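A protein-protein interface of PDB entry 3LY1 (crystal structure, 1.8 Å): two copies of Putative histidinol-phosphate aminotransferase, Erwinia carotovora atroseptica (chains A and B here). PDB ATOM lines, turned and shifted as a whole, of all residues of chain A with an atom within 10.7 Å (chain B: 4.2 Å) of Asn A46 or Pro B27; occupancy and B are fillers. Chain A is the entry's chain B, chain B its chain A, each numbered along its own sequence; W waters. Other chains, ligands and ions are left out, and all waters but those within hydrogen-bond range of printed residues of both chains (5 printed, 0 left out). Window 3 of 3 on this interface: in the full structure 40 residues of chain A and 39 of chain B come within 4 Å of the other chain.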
ATOM      1  N   ALA A  38     -11.049 -19.660   0.857  1.00  0.00           N
ATOM      2  CA  ALA A  38      -9.910 -20.083   1.684  1.00  0.00           C
ATOM      3  C   ALA A  38     -10.084 -19.667   3.130  1.00  0.00           C
ATOM      4  O   ALA A  38      -9.892 -20.479   4.015  1.00  0.00           O
ATOM      5  CB  ALA A  38      -8.582 -19.540   1.137  1.00  0.00           C
ATOM      6  N   ARG A  39     -10.480 -18.407   3.361  1.00  0.00           N
ATOM      7  CA  ARG A  39     -10.665 -17.889   4.700  1.00  0.00           C
ATOM      8  C   ARG A  39     -11.885 -18.516   5.381  1.00  0.00           C
ATOM      9  O   ARG A  39     -11.851 -18.813   6.582  1.00  0.00           O
ATOM     10  CB  ARG A  39     -10.795 -16.363   4.659  1.00  0.00           C
ATOM     11  CG  ARG A  39      -9.472 -15.647   4.389  1.00  0.00           C
ATOM     12  CD  ARG A  39      -9.551 -14.154   4.786  1.00  0.00           C
ATOM     13  NE  ARG A  39     -10.276 -13.410   3.771  1.00  0.00           N
ATOM     14  CZ  ARG A  39      -9.730 -12.901   2.660  1.00  0.00           C
ATOM     15  NH1 ARG A  39      -8.409 -12.993   2.395  1.00  0.00           N
ATOM     16  NH2 ARG A  39     -10.520 -12.288   1.788  1.00  0.00           N
ATOM     17  N   ASP A  40     -12.965 -18.724   4.632  1.00  0.00           N
ATOM     18  CA  ASP A  40     -14.166 -19.353   5.189  1.00  0.00           C
ATOM     19  C   ASP A  40     -13.916 -20.818   5.605  1.00  0.00           C
ATOM     20  O   ASP A  40     -14.561 -21.330   6.520  1.00  0.00           O
ATOM     21  CB  ASP A  40     -15.316 -19.325   4.181  1.00  0.00           C
ATOM     22  CG  ASP A  40     -16.025 -17.978   4.094  1.00  0.00           C
ATOM     23  OD1 ASP A  40     -15.606 -16.951   4.728  1.00  0.00           O
ATOM     24  OD2 ASP A  40     -17.048 -17.977   3.359  1.00  0.00           O
ATOM     25  N   ALA A  41     -12.954 -21.475   4.951  1.00  0.00           N
ATOM     26  CA  ALA A  41     -12.647 -22.852   5.243  1.00  0.00           C
ATOM     27  C   ALA A  41     -11.945 -23.052   6.580  1.00  0.00           C
ATOM     28  O   ALA A  41     -11.926 -24.163   7.080  1.00  0.00           O
ATOM     29  CB  ALA A  41     -11.786 -23.475   4.097  1.00  0.00           C
ATOM     30  N   VAL A  42     -11.387 -21.992   7.172  1.00  0.00           N
ATOM     31  CA  VAL A  42     -10.584 -22.126   8.381  1.00  0.00           C
ATOM     32  C   VAL A  42     -11.407 -22.669   9.546  1.00  0.00           C
ATOM     33  O   VAL A  42     -10.960 -23.555  10.273  1.00  0.00           O
ATOM     34  CB  VAL A  42      -9.890 -20.774   8.747  1.00  0.00           C
ATOM     35  CG1 VAL A  42      -9.281 -20.846  10.119  1.00  0.00           C
ATOM     36  CG2 VAL A  42      -8.763 -20.460   7.699  1.00  0.00           C
ATOM     37  N   VAL A  43     -12.606 -22.125   9.749  1.00  0.00           N
ATOM     38  CA  VAL A  43     -13.511 -22.591  10.802  1.00  0.00           C
ATOM     39  C   VAL A  43     -13.938 -24.070  10.591  1.00  0.00           C
ATOM     40  O   VAL A  43     -14.310 -24.747  11.542  1.00  0.00           O
ATOM     41  CB  VAL A  43     -14.755 -21.597  10.951  1.00  0.00           C
ATOM     42  CG1 VAL A  43     -15.759 -21.799   9.803  1.00  0.00           C
ATOM     43  CG2 VAL A  43     -15.436 -21.701  12.367  1.00  0.00           C
ATOM     44  N   LYS A  44     -13.891 -24.558   9.359  1.00  0.00           N
ATOM     45  CA  LYS A  44     -14.184 -25.966   9.057  1.00  0.00           C
ATOM     46  C   LYS A  44     -12.988 -26.888   9.193  1.00  0.00           C
ATOM     47  O   LYS A  44     -13.150 -28.126   9.169  1.00  0.00           O
ATOM     48  CB  LYS A  44     -14.737 -26.110   7.630  1.00  0.00           C
ATOM     49  CG  LYS A  44     -16.039 -25.323   7.375  1.00  0.00           C
ATOM     50  CD  LYS A  44     -16.634 -25.578   5.971  1.00  0.00           C
ATOM     51  CE  LYS A  44     -15.732 -25.143   4.864  1.00  0.00           C
ATOM     52  NZ  LYS A  44     -16.368 -25.201   3.499  1.00  0.00           N
ATOM     53  N   ALA A  45     -11.784 -26.319   9.300  1.00  0.00           N
ATOM     54  CA  ALA A  45     -10.562 -27.126   9.138  1.00  0.00           C
ATOM     55  C   ALA A  45     -10.111 -27.882  10.380  1.00  0.00           C
ATOM     56  O   ALA A  45      -9.004 -28.452  10.364  1.00  0.00           O
ATOM     57  CB  ALA A  45      -9.407 -26.303   8.530  1.00  0.00           C
ATOM     58  N   ASN A  46     -10.956 -27.960  11.416  1.00  0.00           N
ATOM     59  CA  ASN A  46     -10.797 -28.991  12.451  1.00  0.00           C
ATOM     60  C   ASN A  46     -11.104 -30.404  11.924  1.00  0.00           C
ATOM     61  O   ASN A  46     -10.726 -31.395  12.556  1.00  0.00           O
ATOM     62  CB  ASN A  46     -11.582 -28.699  13.727  1.00  0.00           C
ATOM     63  CG  ASN A  46     -13.088 -28.541  13.480  1.00  0.00           C
ATOM     64  OD1 ASN A  46     -13.481 -27.768  12.609  1.00  0.00           O
ATOM     65  ND2 ASN A  46     -13.919 -29.291  14.225  1.00  0.00           N
ATOM     66  N   ARG A  47     -11.761 -30.462  10.760  1.00  0.00           N
ATOM     67  CA  ARG A  47     -12.118 -31.692  10.085  1.00  0.00           C
ATOM     68  C   ARG A  47     -11.405 -31.833   8.770  1.00  0.00           C
ATOM     69  O   ARG A  47     -11.038 -30.865   8.138  1.00  0.00           O
ATOM     70  CB  ARG A  47     -13.629 -31.696   9.837  1.00  0.00           C
ATOM     71  CG  ARG A  47     -14.405 -31.403  11.108  1.00  0.00           C
ATOM     72  CD  ARG A  47     -15.789 -32.032  11.138  1.00  0.00           C
ATOM     73  NE  ARG A  47     -16.445 -31.721  12.420  1.00  0.00           N
ATOM     74  CZ  ARG A  47     -16.501 -32.541  13.474  1.00  0.00           C
ATOM     75  NH1 ARG A  47     -15.951 -33.769  13.464  1.00  0.00           N
ATOM     76  NH2 ARG A  47     -17.102 -32.128  14.567  1.00  0.00           N
ATOM     77  N   TYR A  48     -11.238 -33.074   8.352  1.00  0.00           N
ATOM     78  CA  TYR A  48     -10.672 -33.367   7.048  1.00  0.00           C
ATOM     79  C   TYR A  48     -11.679 -32.979   5.923  1.00  0.00           C
ATOM     80  O   TYR A  48     -12.869 -33.221   6.038  1.00  0.00           O
ATOM     81  CB  TYR A  48     -10.366 -34.861   6.967  1.00  0.00           C
ATOM     82  CG  TYR A  48      -9.378 -35.350   7.982  1.00  0.00           C
ATOM     83  CD1 TYR A  48      -8.025 -35.150   7.793  1.00  0.00           C
ATOM     84  CD2 TYR A  48      -9.785 -36.049   9.123  1.00  0.00           C
ATOM     85  CE1 TYR A  48      -7.115 -35.621   8.683  1.00  0.00           C
ATOM     86  CE2 TYR A  48      -8.858 -36.516  10.043  1.00  0.00           C
ATOM     87  CZ  TYR A  48      -7.514 -36.279   9.826  1.00  0.00           C
ATOM     88  OH  TYR A  48      -6.537 -36.717  10.723  1.00  0.00           O
ATOM     89  N   ALA A  49     -11.171 -32.410   4.841  1.00  0.00           N
ATOM     90  CA  ALA A  49     -11.970 -32.007   3.658  1.00  0.00           C
ATOM     91  C   ALA A  49     -12.357 -33.186   2.745  1.00  0.00           C
ATOM     92  O   ALA A  49     -12.163 -33.119   1.514  1.00  0.00           O
ATOM     93  CB  ALA A  49     -11.162 -31.008   2.858  1.00  0.00           C
ATOM     94  N   LYS A  50     -12.916 -34.243   3.313  1.00  0.00           N
ATOM     95  CA  LYS A  50     -13.037 -35.508   2.556  1.00  0.00           C
ATOM     96  C   LYS A  50     -13.980 -35.323   1.377  1.00  0.00           C
ATOM     97  O   LYS A  50     -13.580 -35.587   0.217  1.00  0.00           O
ATOM     98  CB  LYS A  50     -13.453 -36.679   3.443  1.00  0.00           C
ATOM     99  CG  LYS A  50     -12.282 -37.349   4.181  1.00  0.00           C
ATOM    100  CD  LYS A  50     -12.811 -38.255   5.267  1.00  0.00           C
ATOM    101  CE  LYS A  50     -11.744 -38.653   6.259  1.00  0.00           C
ATOM    102  NZ  LYS A  50     -10.953 -39.694   5.631  1.00  0.00           N
ATOM    103  N   GLU A  52     -15.087 -32.562  -0.034  1.00  0.00           N
ATOM    104  CA  GLU A  52     -14.642 -31.458  -0.873  1.00  0.00           C
ATOM    105  C   GLU A  52     -13.546 -31.905  -1.846  1.00  0.00           C
ATOM    106  O   GLU A  52     -13.495 -31.455  -2.973  1.00  0.00           O
ATOM    107  CB  GLU A  52     -14.136 -30.349   0.015  1.00  0.00           C
ATOM    108  CG  GLU A  52     -15.220 -29.704   0.906  1.00  0.00           C
ATOM    109  CD  GLU A  52     -15.645 -30.495   2.139  1.00  0.00           C
ATOM    110  OE1 GLU A  52     -14.975 -31.442   2.585  1.00  0.00           O
ATOM    111  OE2 GLU A  52     -16.709 -30.150   2.704  1.00  0.00           O
ATOM    112  N   ILE A 244      -5.607 -33.056   0.757  1.00  0.00           N
ATOM    113  CA  ILE A 244      -5.260 -31.673   0.512  1.00  0.00           C
ATOM    114  C   ILE A 244      -5.900 -30.832   1.598  1.00  0.00           C
ATOM    115  O   ILE A 244      -6.940 -31.194   2.135  1.00  0.00           O
ATOM    116  CB  ILE A 244      -5.840 -31.259  -0.873  1.00  0.00           C
ATOM    117  CG1 ILE A 244      -5.360 -32.238  -1.936  1.00  0.00           C
ATOM    118  CG2 ILE A 244      -5.433 -29.881  -1.266  1.00  0.00           C
ATOM    119  CD1 ILE A 244      -3.815 -32.445  -1.901  1.00  0.00           C
ATOM    120  N   ASN A 245      -5.289 -29.696   1.898  1.00  0.00           N
ATOM    121  CA  ASN A 245      -5.774 -28.848   2.988  1.00  0.00           C
ATOM    122  C   ASN A 245      -7.081 -28.155   2.643  1.00  0.00           C
ATOM    123  O   ASN A 245      -7.329 -27.835   1.472  1.00  0.00           O
ATOM    124  CB  ASN A 245      -4.699 -27.883   3.462  1.00  0.00           C
ATOM    125  CG  ASN A 245      -4.615 -26.628   2.646  1.00  0.00           C
ATOM    126  OD1 ASN A 245      -5.320 -25.634   2.921  1.00  0.00           O
ATOM    127  ND2 ASN A 245      -3.737 -26.640   1.642  1.00  0.00           N
ATOM    128  N   PHE A 246      -7.919 -27.953   3.658  1.00  0.00           N
ATOM    129  CA  PHE A 246      -9.272 -27.400   3.454  1.00  0.00           C
ATOM    130  C   PHE A 246      -9.307 -26.046   2.748  1.00  0.00           C
ATOM    131  O   PHE A 246     -10.113 -25.862   1.825  1.00  0.00           O
ATOM    132  CB  PHE A 246     -10.041 -27.246   4.769  1.00  0.00           C
ATOM    133  CG  PHE A 246     -11.479 -27.773   4.712  1.00  0.00           C
ATOM    134  CD1 PHE A 246     -12.340 -27.422   3.690  1.00  0.00           C
ATOM    135  CD2 PHE A 246     -11.951 -28.609   5.695  1.00  0.00           C
ATOM    136  CE1 PHE A 246     -13.648 -27.908   3.659  1.00  0.00           C
ATOM    137  CE2 PHE A 246     -13.254 -29.089   5.676  1.00  0.00           C
ATOM    138  CZ  PHE A 246     -14.099 -28.741   4.655  1.00  0.00           C
ATOM    139  N   SER A 247      -8.455 -25.105   3.153  1.00  0.00           N
ATOM    140  CA  SER A 247      -8.419 -23.822   2.478  1.00  0.00           C
ATOM    141  C   SER A 247      -8.049 -23.899   1.004  1.00  0.00           C
ATOM    142  O   SER A 247      -8.631 -23.180   0.191  1.00  0.00           O
ATOM    143  CB  SER A 247      -7.523 -22.819   3.217  1.00  0.00           C
ATOM    144  OG  SER A 247      -8.045 -22.574   4.517  1.00  0.00           O
ATOM    145  N   GLU B  25     -11.662 -36.460  14.799  1.00  0.00           N
ATOM    146  CA  GLU B  25     -11.407 -35.035  14.642  1.00  0.00           C
ATOM    147  C   GLU B  25     -11.758 -34.376  15.955  1.00  0.00           C
ATOM    148  O   GLU B  25     -12.635 -34.848  16.677  1.00  0.00           O
ATOM    149  CB  GLU B  25     -12.239 -34.459  13.482  1.00  0.00           C
ATOM    150  CG  GLU B  25     -11.977 -35.216  12.155  1.00  0.00           C
ATOM    151  CD  GLU B  25     -13.123 -35.132  11.148  1.00  0.00           C
ATOM    152  OE1 GLU B  25     -14.307 -35.285  11.544  1.00  0.00           O
ATOM    153  OE2 GLU B  25     -12.828 -34.951   9.943  1.00  0.00           O
ATOM    154  N   ASN B  26     -11.086 -33.273  16.276  1.00  0.00           N
ATOM    155  CA  ASN B  26     -11.392 -32.493  17.455  1.00  0.00           C
ATOM    156  C   ASN B  26     -12.677 -31.749  17.096  1.00  0.00           C
ATOM    157  O   ASN B  26     -12.728 -31.179  15.998  1.00  0.00           O
ATOM    158  CB  ASN B  26     -10.266 -31.495  17.724  1.00  0.00           C
ATOM    159  CG  ASN B  26     -10.334 -30.863  19.097  1.00  0.00           C
ATOM    160  OD1 ASN B  26     -11.406 -30.414  19.557  1.00  0.00           O
ATOM    161  ND2 ASN B  26      -9.180 -30.769  19.749  1.00  0.00           N
ATOM    162  N   PRO B  27     -13.728 -31.828  17.961  1.00  0.00           N
ATOM    163  CA  PRO B  27     -15.052 -31.227  17.695  1.00  0.00           C
ATOM    164  C   PRO B  27     -15.085 -29.731  17.989  1.00  0.00           C
ATOM    165  O   PRO B  27     -16.054 -29.039  17.625  1.00  0.00           O
ATOM    166  CB  PRO B  27     -15.975 -31.972  18.665  1.00  0.00           C
ATOM    167  CG  PRO B  27     -15.082 -32.260  19.850  1.00  0.00           C
ATOM    168  CD  PRO B  27     -13.736 -32.599  19.223  1.00  0.00           C
ATOM    169  N   LEU B  28     -14.025 -29.258  18.633  1.00  0.00           N
ATOM    170  CA  LEU B  28     -13.791 -27.862  18.826  1.00  0.00           C
ATOM    171  C   LEU B  28     -13.208 -27.229  17.574  1.00  0.00           C
ATOM    172  O   LEU B  28     -12.420 -27.841  16.853  1.00  0.00           O
ATOM    173  CB  LEU B  28     -12.801 -27.667  19.966  1.00  0.00           C
ATOM    174  CG  LEU B  28     -13.258 -28.152  21.336  1.00  0.00           C
ATOM    175  CD1 LEU B  28     -12.198 -27.812  22.371  1.00  0.00           C
ATOM    176  CD2 LEU B  28     -14.593 -27.504  21.666  1.00  0.00           C
ATOM    177  N   GLY B  29     -13.577 -25.981  17.318  1.00  0.00           N
ATOM    178  CA  GLY B  29     -12.821 -25.226  16.350  1.00  0.00           C
ATOM    179  C   GLY B  29     -11.368 -25.300  16.771  1.00  0.00           C
ATOM    180  O   GLY B  29     -11.060 -25.564  17.932  1.00  0.00           O
ATOM    181  N   ALA B 216      -6.488 -29.483  16.892  1.00  0.00           N
ATOM    182  CA  ALA B 216      -7.743 -29.288  16.142  1.00  0.00           C
ATOM    183  C   ALA B 216      -7.563 -28.770  14.702  1.00  0.00           C
ATOM    184  O   ALA B 216      -8.398 -28.030  14.212  1.00  0.00           O
ATOM    185  CB  ALA B 216      -8.709 -28.351  16.937  1.00  0.00           C
ATOM    186  N   ALA B 218      -6.919 -30.854  11.745  1.00  0.00           N
ATOM    187  CA  ALA B 218      -6.902 -31.968  10.799  1.00  0.00           C
ATOM    188  C   ALA B 218      -6.886 -31.451   9.358  1.00  0.00           C
ATOM    189  O   ALA B 218      -6.076 -31.871   8.601  1.00  0.00           O
ATOM    190  CB  ALA B 218      -8.103 -32.942  11.023  1.00  0.00           C
ATOM    191  N   LEU B 332     -15.004 -38.826  20.333  1.00  0.00           N
ATOM    192  CA  LEU B 332     -15.605 -37.979  21.349  1.00  0.00           C
ATOM    193  C   LEU B 332     -15.941 -36.619  20.752  1.00  0.00           C
ATOM    194  O   LEU B 332     -15.069 -35.900  20.279  1.00  0.00           O
ATOM    195  CB  LEU B 332     -14.717 -37.890  22.568  1.00  0.00           C
ATOM    196  CG  LEU B 332     -14.472 -39.190  23.346  1.00  0.00           C
ATOM    197  CD1 LEU B 332     -13.483 -38.962  24.525  1.00  0.00           C
ATOM    198  CD2 LEU B 332     -15.765 -39.812  23.851  1.00  0.00           C
ATOM    199  N   GLY B 333     -17.238 -36.328  20.706  1.00  0.00           N
ATOM    200  CA  GLY B 333     -17.752 -35.017  20.304  1.00  0.00           C
ATOM    201  C   GLY B 333     -17.722 -34.010  21.436  1.00  0.00           C
ATOM    202  O   GLY B 333     -17.110 -34.240  22.475  1.00  0.00           O
ATOM    203  N   THR B 334     -18.388 -32.872  21.241  1.00  0.00           N
ATOM    204  CA  THR B 334     -18.468 -31.859  22.294  1.00  0.00           C
ATOM    205  C   THR B 334     -19.309 -32.471  23.417  1.00  0.00           C
ATOM    206  O   THR B 334     -20.024 -33.452  23.166  1.00  0.00           O
ATOM    207  CB  THR B 334     -19.153 -30.557  21.820  1.00  0.00           C
ATOM    208  OG1 THR B 334     -20.542 -30.804  21.539  1.00  0.00           O
ATOM    209  CG2 THR B 334     -18.454 -29.993  20.576  1.00  0.00           C
ATOM    210  N   GLU B 337     -22.849 -32.715  22.416  1.00  0.00           N
ATOM    211  CA  GLU B 337     -23.088 -33.770  21.435  1.00  0.00           C
ATOM    212  C   GLU B 337     -23.121 -35.151  22.117  1.00  0.00           C
ATOM    213  O   GLU B 337     -23.910 -36.030  21.729  1.00  0.00           O
ATOM    214  CB  GLU B 337     -22.052 -33.741  20.308  1.00  0.00           C
ATOM    215  CG  GLU B 337     -22.186 -32.582  19.313  1.00  0.00           C
ATOM    216  CD  GLU B 337     -21.012 -32.516  18.321  1.00  0.00           C
ATOM    217  OE1 GLU B 337     -19.896 -33.020  18.635  1.00  0.00           O
ATOM    218  OE2 GLU B 337     -21.213 -31.951  17.223  1.00  0.00           O
HETATM  219  O   HOH W   1     -15.538 -35.725  15.924  1.00  0.00           O
HETATM  220  O   HOH W   2     -14.220 -35.182   7.560  1.00  0.00           O
HETATM  221  O   HOH W   3     -18.458 -30.048  16.355  1.00  0.00           O
HETATM  222  O   HOH W   4      -9.172 -31.941  14.577  1.00  0.00           O
HETATM  223  O   HOH W   5     -18.122 -33.921  16.635  1.00  0.00           O
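OE1 of Glu B25 is in salt-bridge range of NH1 of Arg A47 (2.9 Å).
N of Tyr A48 is in hydrogen-bond range of OE2 of Glu B25 (2.9 Å).
The side-chain amide nitrogen (ND2) of Asn A46 is in hydrogen-bond range of the backbone carbonyl oxygen (O) of Asn B26.
ND2 of Asn A46 lies close to O of Leu B28, at 3.4 Å.
N of Ala B218 sits at hydrogen-bond distance from O of Ala A45 (3.5 Å).
The backbone NH (N) of Leu B28 is in hydrogen-bond range of the side-chain amide oxygen (OD1) of Asn B26 (3.0 Å).
The backbone carbonyl oxygen (O) of Val A43 lies close to the side-chain amide oxygen (OD1) of Asn A46 (3.3 Å).
The side-chain amide oxygen of Asn A46 lies close to the backbone carbonyl oxygen of Lys A44 (3.5 Å).
Among the printed residues, merely in contact across the chains: Asn A46 with Ala B216 (3.1 Å), Asn A46 with Ala B218 (3.4 Å), Asn A46 with Glu B25 (3.5 Å), Tyr A48 with Ala B218 (3.6 Å), Arg A47 with Pro B27 (3.8 Å), Ala A45 with Ala B216 (3.9 Å) and Asn A46 with Pro B27 (3.96 Å).
Pro B27 touches two residues of chain A.
Glu B25 touches just these residues of chain A: Asn A46 (3.5 Å), Arg A47 (2.9 Å) and Tyr A48 (2.9 Å).
Asn B26 touches just one residue of chain A: Asn A46.
Printed residues of chain A within 4 Å of Ala B218: Ala A45, Asn A46 and Tyr A48.
Printed residues of chain B within 4 Å of Tyr A48: Glu B25 (2.9 Å) and Ala B218 (3.6 Å).
Of the printed residues of chain A, Leu B28 touches Asn A46 (3.3 Å).
Printed residues of chain B within 4 Å of Ala A45: Ala B216 (3.9 Å) and Ala B218 (3.5 Å).
Lys A44 touches none of the printed residues of chain B.
The nearest residue of chain A that does not touch Pro B27 is Val A43 (7.6 Å).
The nearest printed residue of chain B that does not touch Ala A45 is Leu B28 (6.9 Å).
Hydrophobic or aromatic side chains of chain B that line the printed part of chain A: Ala B218.
Of the 18 printed residues of chain A, 4 touch a printed residue of chain B.
Hydrophobic or aromatic side chains of chain A within 4 Å of the printed part of chain B: Tyr A48.
Among the printed residues, 12 pairs touch across the chains.
Among the printed residues, Asp or Glu carboxylates within 4 Å of a Lys or Arg side-chain nitrogen of the other chain: Arg A47 with Glu B25 (2.9 Å).
No position is printed for both chains.
Of the 12 pairs that touch across the chains among the printed residues, none has its exchanged pair printed and touching as well.
Water W4 bridges O of Asn A46 (2.6 Å) and N of Asn B26 (2.9 Å).
Water W2 lies within hydrogen-bond range of OE2 of Glu B25 (2.8 Å) and O of Tyr A48 (2.8 Å).
Water W5 lies within hydrogen-bond range of the side-chain carboxylate of Glu B337 and the guanidinium group of Arg A47.
Water W3 lies within hydrogen-bond range of O of Pro B27, NH2 of Arg A47 and OE2 of Glu B337.
Water W1 lies within hydrogen-bond range of the backbone carbonyl oxygen (O) of Glu B25 (3.1 Å) and the guanidinium group (NH1) of Arg A47 (3.2 Å).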
